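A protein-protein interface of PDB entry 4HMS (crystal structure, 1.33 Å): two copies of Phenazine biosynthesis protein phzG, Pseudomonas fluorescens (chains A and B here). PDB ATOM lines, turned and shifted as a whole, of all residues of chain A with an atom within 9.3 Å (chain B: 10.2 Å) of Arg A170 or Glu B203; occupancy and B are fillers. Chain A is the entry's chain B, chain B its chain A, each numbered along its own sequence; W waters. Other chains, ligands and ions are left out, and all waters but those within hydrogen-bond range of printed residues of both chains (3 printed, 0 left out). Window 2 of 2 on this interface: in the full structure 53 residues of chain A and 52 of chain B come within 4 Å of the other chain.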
ATOM      1  N   ALA A 145       6.229  -8.039 -10.343  1.00  0.00           N
ATOM      2  CA  ALA A 145       5.576  -8.955 -11.294  1.00  0.00           C
ATOM      3  C   ALA A 145       6.123 -10.364 -11.237  1.00  0.00           C
ATOM      4  O   ALA A 145       5.461 -11.294 -11.711  1.00  0.00           O
ATOM      5  CB  ALA A 145       5.707  -8.447 -12.718  1.00  0.00           C
ATOM      6  N   THR A 146       7.320 -10.535 -10.678  1.00  0.00           N
ATOM      7  CA  THR A 146       7.883 -11.875 -10.535  1.00  0.00           C
ATOM      8  C   THR A 146       7.360 -12.594  -9.294  1.00  0.00           C
ATOM      9  O   THR A 146       7.513 -13.820  -9.151  1.00  0.00           O
ATOM     10  CB  THR A 146       9.426 -11.829 -10.469  1.00  0.00           C
ATOM     11  OG1 THR A 146       9.841 -11.259  -9.221  1.00  0.00           O
ATOM     12  CG2 THR A 146      10.000 -11.020 -11.628  1.00  0.00           C
ATOM     13  N   HIS A 147       6.712 -11.863  -8.386  1.00  0.00           N
ATOM     14  CA  HIS A 147       6.361 -12.482  -7.116  1.00  0.00           C
ATOM     15  C   HIS A 147       5.253 -13.569  -7.176  1.00  0.00           C
ATOM     16  O   HIS A 147       5.365 -14.595  -6.490  1.00  0.00           O
ATOM     17  CB  HIS A 147       5.984 -11.434  -6.050  1.00  0.00           C
ATOM     18  CG  HIS A 147       7.124 -10.564  -5.590  1.00  0.00           C
ATOM     19  ND1 HIS A 147       6.953  -9.582  -4.642  1.00  0.00           N
ATOM     20  CD2 HIS A 147       8.443 -10.550  -5.905  1.00  0.00           C
ATOM     21  CE1 HIS A 147       8.105  -8.975  -4.419  1.00  0.00           C
ATOM     22  NE2 HIS A 147       9.033  -9.564  -5.149  1.00  0.00           N
ATOM     23  N   PRO A 148       4.196 -13.347  -7.977  1.00  0.00           N
ATOM     24  CA  PRO A 148       3.116 -14.352  -7.947  1.00  0.00           C
ATOM     25  C   PRO A 148       3.576 -15.765  -8.336  1.00  0.00           C
ATOM     26  O   PRO A 148       3.326 -16.713  -7.570  1.00  0.00           O
ATOM     27  CB  PRO A 148       2.091 -13.811  -8.955  1.00  0.00           C
ATOM     28  CG  PRO A 148       2.252 -12.277  -8.821  1.00  0.00           C
ATOM     29  CD  PRO A 148       3.804 -12.116  -8.712  1.00  0.00           C
ATOM     30  N   MET A 149       4.287 -15.920  -9.457  1.00  0.00           N
ATOM     31  CA  MET A 149       4.647 -17.271  -9.893  1.00  0.00           C
ATOM     32  C   MET A 149       5.698 -17.877  -8.949  1.00  0.00           C
ATOM     33  O   MET A 149       5.654 -19.064  -8.632  1.00  0.00           O
ATOM     34  CB  MET A 149       5.142 -17.315 -11.343  1.00  0.00           C
ATOM     35  CG  MET A 149       5.169 -18.750 -11.879  1.00  0.00           C
ATOM     36  SD  MET A 149       3.520 -19.472 -12.077  1.00  0.00           S
ATOM     37  CE  MET A 149       2.810 -18.318 -13.260  1.00  0.00           C
ATOM     38  N   SER A 150       6.619 -17.057  -8.474  1.00  0.00           N
ATOM     39  CA  SER A 150       7.660 -17.540  -7.574  1.00  0.00           C
ATOM     40  C   SER A 150       7.098 -17.927  -6.221  1.00  0.00           C
ATOM     41  O   SER A 150       7.743 -18.659  -5.472  1.00  0.00           O
ATOM     42  CB  SER A 150       8.706 -16.457  -7.396  1.00  0.00           C
ATOM     43  OG  SER A 150       9.466 -16.270  -8.577  1.00  0.00           O
ATOM     44  N   VAL A 152       3.747 -19.253  -5.893  1.00  0.00           N
ATOM     45  CA  VAL A 152       2.896 -20.437  -6.051  1.00  0.00           C
ATOM     46  C   VAL A 152       3.726 -21.669  -6.411  1.00  0.00           C
ATOM     47  O   VAL A 152       3.401 -22.785  -6.020  1.00  0.00           O
ATOM     48  CB  VAL A 152       1.727 -20.218  -7.085  1.00  0.00           C
ATOM     49  CG1 VAL A 152       0.790 -19.112  -6.619  1.00  0.00           C
ATOM     50  CG2 VAL A 152       2.243 -19.907  -8.456  1.00  0.00           C
ATOM     51  N   VAL A 162      -0.992 -27.504 -15.226  1.00  0.00           N
ATOM     52  CA  VAL A 162      -0.437 -26.223 -15.676  1.00  0.00           C
ATOM     53  C   VAL A 162      -1.467 -25.102 -15.493  1.00  0.00           C
ATOM     54  O   VAL A 162      -1.150 -24.029 -14.962  1.00  0.00           O
ATOM     55  CB  VAL A 162      -0.007 -26.312 -17.156  1.00  0.00           C
ATOM     56  CG1 VAL A 162       0.463 -24.959 -17.701  1.00  0.00           C
ATOM     57  CG2 VAL A 162       1.074 -27.397 -17.376  1.00  0.00           C
ATOM     58  N   GLN A 163      -2.702 -25.347 -15.902  1.00  0.00           N
ATOM     59  CA  GLN A 163      -3.737 -24.322 -15.813  1.00  0.00           C
ATOM     60  C   GLN A 163      -4.033 -23.929 -14.382  1.00  0.00           C
ATOM     61  O   GLN A 163      -4.246 -22.750 -14.132  1.00  0.00           O
ATOM     62  CB  GLN A 163      -5.003 -24.753 -16.575  1.00  0.00           C
ATOM     63  CG  GLN A 163      -6.008 -23.568 -16.756  1.00  0.00           C
ATOM     64  CD  GLN A 163      -5.429 -22.515 -17.727  1.00  0.00           C
ATOM     65  OE1 GLN A 163      -4.730 -22.867 -18.683  1.00  0.00           O
ATOM     66  NE2 GLN A 163      -5.687 -21.239 -17.465  1.00  0.00           N
ATOM     67  N   ALA A 164      -3.974 -24.864 -13.436  1.00  0.00           N
ATOM     68  CA  ALA A 164      -4.223 -24.526 -12.032  1.00  0.00           C
ATOM     69  C   ALA A 164      -3.153 -23.584 -11.499  1.00  0.00           C
ATOM     70  O   ALA A 164      -3.437 -22.650 -10.742  1.00  0.00           O
ATOM     71  CB  ALA A 164      -4.253 -25.758 -11.156  1.00  0.00           C
ATOM     72  N   MET A 165      -1.897 -23.831 -11.891  1.00  0.00           N
ATOM     73  CA  MET A 165      -0.820 -22.970 -11.421  1.00  0.00           C
ATOM     74  C   MET A 165      -0.961 -21.576 -12.053  1.00  0.00           C
ATOM     75  O   MET A 165      -0.822 -20.540 -11.386  1.00  0.00           O
ATOM     76  CB  MET A 165       0.539 -23.596 -11.735  1.00  0.00           C
ATOM     77  CG  MET A 165       1.688 -22.631 -11.402  1.00  0.00           C
ATOM     78  SD  MET A 165       3.327 -23.350 -11.505  1.00  0.00           S
ATOM     79  CE  MET A 165       3.237 -24.349 -10.019  1.00  0.00           C
ATOM     80  N   ARG A 166      -1.290 -21.555 -13.340  1.00  0.00           N
ATOM     81  CA  ARG A 166      -1.506 -20.305 -14.050  1.00  0.00           C
ATOM     82  C   ARG A 166      -2.631 -19.478 -13.387  1.00  0.00           C
ATOM     83  O   ARG A 166      -2.473 -18.258 -13.141  1.00  0.00           O
ATOM     84  CB  ARG A 166      -1.827 -20.638 -15.503  1.00  0.00           C
ATOM     85  CG  ARG A 166      -1.677 -19.475 -16.443  1.00  0.00           C
ATOM     86  CD  ARG A 166      -1.884 -19.844 -17.916  1.00  0.00           C
ATOM     87  NE  ARG A 166      -0.863 -20.721 -18.495  1.00  0.00           N
ATOM     88  CZ  ARG A 166       0.419 -20.405 -18.717  1.00  0.00           C
ATOM     89  NH1 ARG A 166       0.928 -19.226 -18.383  1.00  0.00           N
ATOM     90  NH2 ARG A 166       1.200 -21.299 -19.270  1.00  0.00           N
ATOM     91  N   ASN A 167      -3.752 -20.138 -13.078  1.00  0.00           N
ATOM     92  CA  ASN A 167      -4.900 -19.440 -12.533  1.00  0.00           C
ATOM     93  C   ASN A 167      -4.619 -18.936 -11.119  1.00  0.00           C
ATOM     94  O   ASN A 167      -5.023 -17.826 -10.747  1.00  0.00           O
ATOM     95  CB  ASN A 167      -6.137 -20.331 -12.575  1.00  0.00           C
ATOM     96  CG  ASN A 167      -6.724 -20.489 -14.011  1.00  0.00           C
ATOM     97  OD1 ASN A 167      -6.392 -19.733 -14.919  1.00  0.00           O
ATOM     98  ND2 ASN A 167      -7.577 -21.491 -14.204  1.00  0.00           N
ATOM     99  N   ALA A 168      -3.915 -19.747 -10.331  1.00  0.00           N
ATOM    100  CA  ALA A 168      -3.542 -19.327  -8.984  1.00  0.00           C
ATOM    101  C   ALA A 168      -2.633 -18.108  -9.010  1.00  0.00           C
ATOM    102  O   ALA A 168      -2.832 -17.172  -8.232  1.00  0.00           O
ATOM    103  CB  ALA A 168      -2.898 -20.472  -8.207  1.00  0.00           C
ATOM    104  N   ALA A 169      -1.613 -18.121  -9.869  1.00  0.00           N
ATOM    105  CA  ALA A 169      -0.711 -16.976  -9.943  1.00  0.00           C
ATOM    106  C   ALA A 169      -1.449 -15.719 -10.404  1.00  0.00           C
ATOM    107  O   ALA A 169      -1.217 -14.630  -9.870  1.00  0.00           O
ATOM    108  CB  ALA A 169       0.476 -17.273 -10.861  1.00  0.00           C
ATOM    109  N   ARG A 170      -2.360 -15.874 -11.358  1.00  0.00           N
ATOM    110  CA  ARG A 170      -3.129 -14.729 -11.850  1.00  0.00           C
ATOM    111  C   ARG A 170      -3.933 -14.085 -10.706  1.00  0.00           C
ATOM    112  O   ARG A 170      -4.030 -12.861 -10.611  1.00  0.00           O
ATOM    113  CB  ARG A 170      -4.072 -15.151 -12.991  1.00  0.00           C
ATOM    114  CG  ARG A 170      -3.389 -15.323 -14.330  1.00  0.00           C
ATOM    115  CD  ARG A 170      -4.417 -15.737 -15.387  1.00  0.00           C
ATOM    116  NE  ARG A 170      -3.786 -15.987 -16.670  1.00  0.00           N
ATOM    117  CZ  ARG A 170      -4.407 -16.564 -17.689  1.00  0.00           C
ATOM    118  NH1 ARG A 170      -5.678 -16.949 -17.551  1.00  0.00           N
ATOM    119  NH2 ARG A 170      -3.761 -16.755 -18.841  1.00  0.00           N
ATOM    120  N   GLN A 171      -4.526 -14.896  -9.832  1.00  0.00           N
ATOM    121  CA  GLN A 171      -5.264 -14.356  -8.706  1.00  0.00           C
ATOM    122  C   GLN A 171      -4.332 -13.568  -7.772  1.00  0.00           C
ATOM    123  O   GLN A 171      -4.709 -12.502  -7.282  1.00  0.00           O
ATOM    124  CB  GLN A 171      -5.959 -15.469  -7.952  1.00  0.00           C
ATOM    125  CG  GLN A 171      -6.904 -14.926  -6.925  1.00  0.00           C
ATOM    126  CD  GLN A 171      -7.993 -14.061  -7.555  1.00  0.00           C
ATOM    127  OE1 GLN A 171      -8.545 -14.406  -8.611  1.00  0.00           O
ATOM    128  NE2 GLN A 171      -8.287 -12.933  -6.929  1.00  0.00           N
ATOM    129  N   LEU A 172      -3.118 -14.069  -7.517  1.00  0.00           N
ATOM    130  CA  LEU A 172      -2.185 -13.312  -6.641  1.00  0.00           C
ATOM    131  C   LEU A 172      -1.707 -12.039  -7.282  1.00  0.00           C
ATOM    132  O   LEU A 172      -1.364 -11.057  -6.604  1.00  0.00           O
ATOM    133  CB  LEU A 172      -0.940 -14.117  -6.278  1.00  0.00           C
ATOM    134  CG  LEU A 172      -1.074 -15.191  -5.245  1.00  0.00           C
ATOM    135  CD1 LEU A 172       0.279 -15.869  -5.018  1.00  0.00           C
ATOM    136  CD2 LEU A 172      -1.636 -14.603  -3.936  1.00  0.00           C
ATOM    137  N   ALA A 173      -1.642 -12.057  -8.602  1.00  0.00           N
ATOM    138  CA  ALA A 173      -1.093 -10.932  -9.343  1.00  0.00           C
ATOM    139  C   ALA A 173      -2.025  -9.754  -9.323  1.00  0.00           C
ATOM    140  O   ALA A 173      -1.628  -8.675  -9.681  1.00  0.00           O
ATOM    141  CB  ALA A 173      -0.801 -11.334 -10.780  1.00  0.00           C
ATOM    142  N   GLU A 174      -3.268  -9.947  -8.901  1.00  0.00           N
ATOM    143  CA  GLU A 174      -4.207  -8.824  -8.886  1.00  0.00           C
ATOM    144  C   GLU A 174      -3.715  -7.680  -7.983  1.00  0.00           C
ATOM    145  O   GLU A 174      -3.988  -6.511  -8.243  1.00  0.00           O
ATOM    146  CB  GLU A 174      -5.583  -9.318  -8.463  1.00  0.00           C
ATOM    147  CG  GLU A 174      -6.202 -10.292  -9.476  1.00  0.00           C
ATOM    148  N   LEU A 175      -2.979  -8.020  -6.935  1.00  0.00           N
ATOM    149  CA  LEU A 175      -2.439  -7.022  -6.007  1.00  0.00           C
ATOM    150  C   LEU A 175      -1.610  -5.925  -6.694  1.00  0.00           C
ATOM    151  O   LEU A 175      -1.680  -4.739  -6.327  1.00  0.00           O
ATOM    152  CB  LEU A 175      -1.580  -7.724  -4.947  1.00  0.00           C
ATOM    153  CG  LEU A 175      -0.958  -6.795  -3.914  1.00  0.00           C
ATOM    154  CD1 LEU A 175      -2.056  -6.106  -3.066  1.00  0.00           C
ATOM    155  CD2 LEU A 175       0.027  -7.569  -3.045  1.00  0.00           C
ATOM    156  N   GLN A 176      -0.813  -6.300  -7.683  1.00  0.00           N
ATOM    157  CA  GLN A 176      -0.038  -5.292  -8.408  1.00  0.00           C
ATOM    158  C   GLN A 176       0.903  -4.553  -7.448  1.00  0.00           C
ATOM    159  O   GLN A 176       1.018  -3.327  -7.495  1.00  0.00           O
ATOM    160  CB  GLN A 176      -0.983  -4.286  -9.101  1.00  0.00           C
ATOM    161  N   LEU A 179       4.611  -9.035  -2.656  1.00  0.00           N
ATOM    162  CA  LEU A 179       4.080 -10.064  -1.802  1.00  0.00           C
ATOM    163  C   LEU A 179       5.148 -10.414  -0.783  1.00  0.00           C
ATOM    164  O   LEU A 179       6.332 -10.124  -0.984  1.00  0.00           O
ATOM    165  CB  LEU A 179       3.793 -11.301  -2.648  1.00  0.00           C
ATOM    166  CG  LEU A 179       2.672 -11.158  -3.670  1.00  0.00           C
ATOM    167  CD1 LEU A 179       2.550 -12.389  -4.530  1.00  0.00           C
ATOM    168  CD2 LEU A 179       1.333 -10.952  -2.989  1.00  0.00           C
ATOM    169  N   GLY B 199      11.905 -23.758 -21.553  1.00  0.00           N
ATOM    170  CA  GLY B 199      11.564 -22.572 -22.311  1.00  0.00           C
ATOM    171  C   GLY B 199      10.951 -21.528 -21.409  1.00  0.00           C
ATOM    172  O   GLY B 199      10.459 -21.830 -20.311  1.00  0.00           O
ATOM    173  N   ASN B 200      10.943 -20.284 -21.855  1.00  0.00           N
ATOM    174  CA  ASN B 200      10.547 -19.182 -20.999  1.00  0.00           C
ATOM    175  C   ASN B 200       9.054 -19.167 -20.698  1.00  0.00           C
ATOM    176  O   ASN B 200       8.650 -18.661 -19.658  1.00  0.00           O
ATOM    177  CB  ASN B 200      10.957 -17.835 -21.646  1.00  0.00           C
ATOM    178  CG  ASN B 200      10.840 -16.658 -20.689  1.00  0.00           C
ATOM    179  OD1 ASN B 200      11.350 -16.666 -19.575  1.00  0.00           O
ATOM    180  ND2 ASN B 200      10.139 -15.634 -21.143  1.00  0.00           N
ATOM    181  N   GLY B 201       8.241 -19.728 -21.597  1.00  0.00           N
ATOM    182  CA  GLY B 201       6.802 -19.795 -21.348  1.00  0.00           C
ATOM    183  C   GLY B 201       6.124 -18.449 -21.349  1.00  0.00           C
ATOM    184  O   GLY B 201       6.652 -17.464 -21.861  1.00  0.00           O
ATOM    185  N   GLN B 202       4.914 -18.437 -20.786  1.00  0.00           N
ATOM    186  CA  GLN B 202       4.093 -17.225 -20.705  1.00  0.00           C
ATOM    187  C   GLN B 202       3.799 -16.919 -19.240  1.00  0.00           C
ATOM    188  O   GLN B 202       3.630 -17.846 -18.436  1.00  0.00           O
ATOM    189  CB  GLN B 202       2.773 -17.398 -21.457  1.00  0.00           C
ATOM    190  CG  GLN B 202       2.921 -17.474 -22.966  1.00  0.00           C
ATOM    191  CD  GLN B 202       3.391 -18.832 -23.420  1.00  0.00           C
ATOM    192  OE1 GLN B 202       4.378 -18.955 -24.150  1.00  0.00           O
ATOM    193  NE2 GLN B 202       2.683 -19.874 -22.980  1.00  0.00           N
ATOM    194  N   GLU B 203       3.744 -15.626 -18.897  1.00  0.00           N
ATOM    195  CA  GLU B 203       3.423 -15.182 -17.528  1.00  0.00           C
ATOM    196  C   GLU B 203       4.360 -15.738 -16.480  1.00  0.00           C
ATOM    197  O   GLU B 203       3.976 -15.957 -15.342  1.00  0.00           O
ATOM    198  CB  GLU B 203       1.997 -15.587 -17.143  1.00  0.00           C
ATOM    199  CG  GLU B 203       0.929 -15.156 -18.118  1.00  0.00           C
ATOM    200  CD  GLU B 203      -0.396 -15.832 -17.805  1.00  0.00           C
ATOM    201  OE1 GLU B 203      -1.060 -15.409 -16.835  1.00  0.00           O
ATOM    202  OE2 GLU B 203      -0.755 -16.804 -18.512  1.00  0.00           O
ATOM    203  N   ARG B 204       5.594 -15.957 -16.891  1.00  0.00           N
ATOM    204  CA  ARG B 204       6.647 -16.483 -16.019  1.00  0.00           C
ATOM    205  C   ARG B 204       6.443 -17.938 -15.598  1.00  0.00           C
ATOM    206  O   ARG B 204       7.220 -18.467 -14.738  1.00  0.00           O
ATOM    207  CB  ARG B 204       6.845 -15.580 -14.798  1.00  0.00           C
ATOM    208  CG  ARG B 204       7.033 -14.107 -15.166  1.00  0.00           C
ATOM    209  CD  ARG B 204       7.771 -13.335 -14.067  1.00  0.00           C
ATOM    210  NE  ARG B 204       9.143 -13.817 -13.873  1.00  0.00           N
ATOM    211  CZ  ARG B 204      10.214 -13.332 -14.502  1.00  0.00           C
ATOM    212  NH1 ARG B 204      10.091 -12.338 -15.369  1.00  0.00           N
ATOM    213  NH2 ARG B 204      11.416 -13.844 -14.266  1.00  0.00           N
ATOM    214  N   LEU B 205       5.453 -18.607 -16.210  1.00  0.00           N
ATOM    215  CA  LEU B 205       5.286 -20.040 -15.980  1.00  0.00           C
ATOM    216  C   LEU B 205       6.249 -20.728 -16.931  1.00  0.00           C
ATOM    217  O   LEU B 205       5.897 -21.183 -18.007  1.00  0.00           O
ATOM    218  CB  LEU B 205       3.847 -20.512 -16.179  1.00  0.00           C
ATOM    219  CG  LEU B 205       3.486 -21.760 -15.361  1.00  0.00           C
ATOM    220  CD1 LEU B 205       1.976 -21.952 -15.364  1.00  0.00           C
ATOM    221  CD2 LEU B 205       4.198 -23.028 -15.873  1.00  0.00           C
ATOM    222  N   HIS B 206       7.506 -20.758 -16.523  1.00  0.00           N
ATOM    223  CA  HIS B 206       8.522 -21.324 -17.374  1.00  0.00           C
ATOM    224  C   HIS B 206       8.184 -22.797 -17.593  1.00  0.00           C
ATOM    225  O   HIS B 206       7.736 -23.502 -16.671  1.00  0.00           O
ATOM    226  CB  HIS B 206       9.895 -21.144 -16.731  1.00  0.00           C
ATOM    227  CG  HIS B 206      10.181 -19.750 -16.325  1.00  0.00           C
ATOM    228  ND1 HIS B 206      10.006 -18.670 -17.170  1.00  0.00           N
ATOM    229  CD2 HIS B 206      10.629 -19.250 -15.151  1.00  0.00           C
ATOM    230  CE1 HIS B 206      10.345 -17.563 -16.527  1.00  0.00           C
ATOM    231  NE2 HIS B 206      10.713 -17.885 -15.300  1.00  0.00           N
ATOM    232  N   GLU B 207       8.473 -23.264 -18.806  1.00  0.00           N
ATOM    233  CA  GLU B 207       8.047 -24.559 -19.267  1.00  0.00           C
ATOM    234  C   GLU B 207       9.204 -25.539 -19.196  1.00  0.00           C
ATOM    235  O   GLU B 207      10.235 -25.337 -19.823  1.00  0.00           O
ATOM    236  CB  GLU B 207       7.525 -24.421 -20.693  1.00  0.00           C
ATOM    237  CG  GLU B 207       6.237 -23.554 -20.671  1.00  0.00           C
ATOM    238  CD  GLU B 207       5.634 -23.217 -22.035  1.00  0.00           C
ATOM    239  OE1 GLU B 207       6.245 -23.529 -23.106  1.00  0.00           O
ATOM    240  OE2 GLU B 207       4.511 -22.646 -22.061  1.00  0.00           O
ATOM    241  N   PRO B 225       8.183 -24.301 -12.210  1.00  0.00           N
ATOM    242  CA  PRO B 225       9.241 -23.348 -12.572  1.00  0.00           C
ATOM    243  C   PRO B 225      10.013 -22.784 -11.421  1.00  0.00           C
ATOM    244  O   PRO B 225      11.172 -22.375 -11.703  1.00  0.00           O
ATOM    245  CB  PRO B 225       8.480 -22.250 -13.308  1.00  0.00           C
ATOM    246  CG  PRO B 225       7.135 -22.315 -12.753  1.00  0.00           C
ATOM    247  CD  PRO B 225       6.853 -23.753 -12.556  1.00  0.00           C
ATOM    248  OXT PRO B 225       9.526 -22.703 -10.266  1.00  0.00           O
HETATM  249  O   HOH W   1       8.562 -15.542 -11.279  1.00  0.00           O
HETATM  250  O   HOH W   2       3.940 -21.049 -19.919  1.00  0.00           O
HETATM  251  O   HOH W   3      -0.505 -16.644 -14.445  1.00  0.00           O
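Hydrophobic or aromatic side chains of chain B within 4 Å of the printed part of chain A: Leu B205 and Pro B225.
Hydrophobic or aromatic side chains of chain A that line the printed part of chain B: Met A149 and Met A165.
The side-chain carboxylate (OE2) of Glu B207 is in hydrogen-bond range of the side-chain amide nitrogen (NE2) of Gln B202 (3.4 Å).
OG of Ser A150 lies within hydrogen-bond range of O of Thr A146, 3.2 Å away.
No position is printed for both chains.
Arg A170 touches just one residue of chain B: Glu B203 (2.8 Å).
Glu B203 touches just these residues of chain A: Met A149 (3.4 Å), Arg A166 (3.0 Å) and Arg A170 (2.8 Å).
No residue of chain B comes within 4 Å of Asn A167.
No residue of chain B comes within 4 Å of Ala A168.
No residue of chain B comes within 4 Å of Ala A169.
No residue of chain B comes within 4 Å of Ala A173.
Printed residues of chain B within 4 Å of Ala A145: Arg B204.
Printed residues of chain B within 4 Å of Thr A146: Arg B204.
Printed residues of chain B within 4 Å of Arg A166: Gln B202, Glu B203 and Leu B205.
Printed residues of chain A within 4 Å of Pro B225: Met A165 (3.7 Å).
Ser A150 touches none of the printed residues of chain B.
The nearest printed residue of chain B that does not touch Arg A170 is Gln B202 (7.1 Å).
The nearest residue of chain A that does not touch Glu B203 is Ala A169 (5.8 Å).
The nearest printed residue of chain A that does not touch Arg B204 is Ser A150 (5.8 Å).
Ala A145 touches Arg B204.
Arg B204 touches Thr A146.
CE of Met A149 touches O of Glu B203, 3.4 Å away.
Arg B204 touches Met A149.
CE of Met A149 touches CB of Leu B205, 3.8 Å away.
CD1 of Leu B205 touches O of Val A162, at 3.8 Å.
Met A165 touches Pro B225 (SD to CD, 3.7 Å).
Leu B205 touches Arg A166 (CD1 to N, 3.9 Å).
The backbone carbonyl oxygen of Gln B202 is in hydrogen-bond range of the guanidinium group of Arg A166 (3.0 Å).
OE2 of Glu B203 lies within salt-bridge range of NH1 of Arg A166 (3.0 Å).
NE of Arg A170 lies within salt-bridge range of OE1 of Glu B203, at 2.8 Å.
Water W2 lies within hydrogen-bond range of the side-chain carboxylate (OE2) of Glu B207, the backbone carbonyl oxygen (O) of Leu B205, the guanidinium group (NH2) of Arg A166 and the backbone NH (N) of Gln B202.
Water W3 bridges OE1 of Glu B203 (2.7 Å) and O of Arg A166 (2.9 Å).
Water W1 lies within hydrogen-bond range of the backbone carbonyl oxygen (O) of Thr A146 (2.9 Å), the side-chain hydroxyl (OG) of Ser A150 (2.9 Å) and the guanidinium group (NE) of Arg B204 (3.2 Å).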
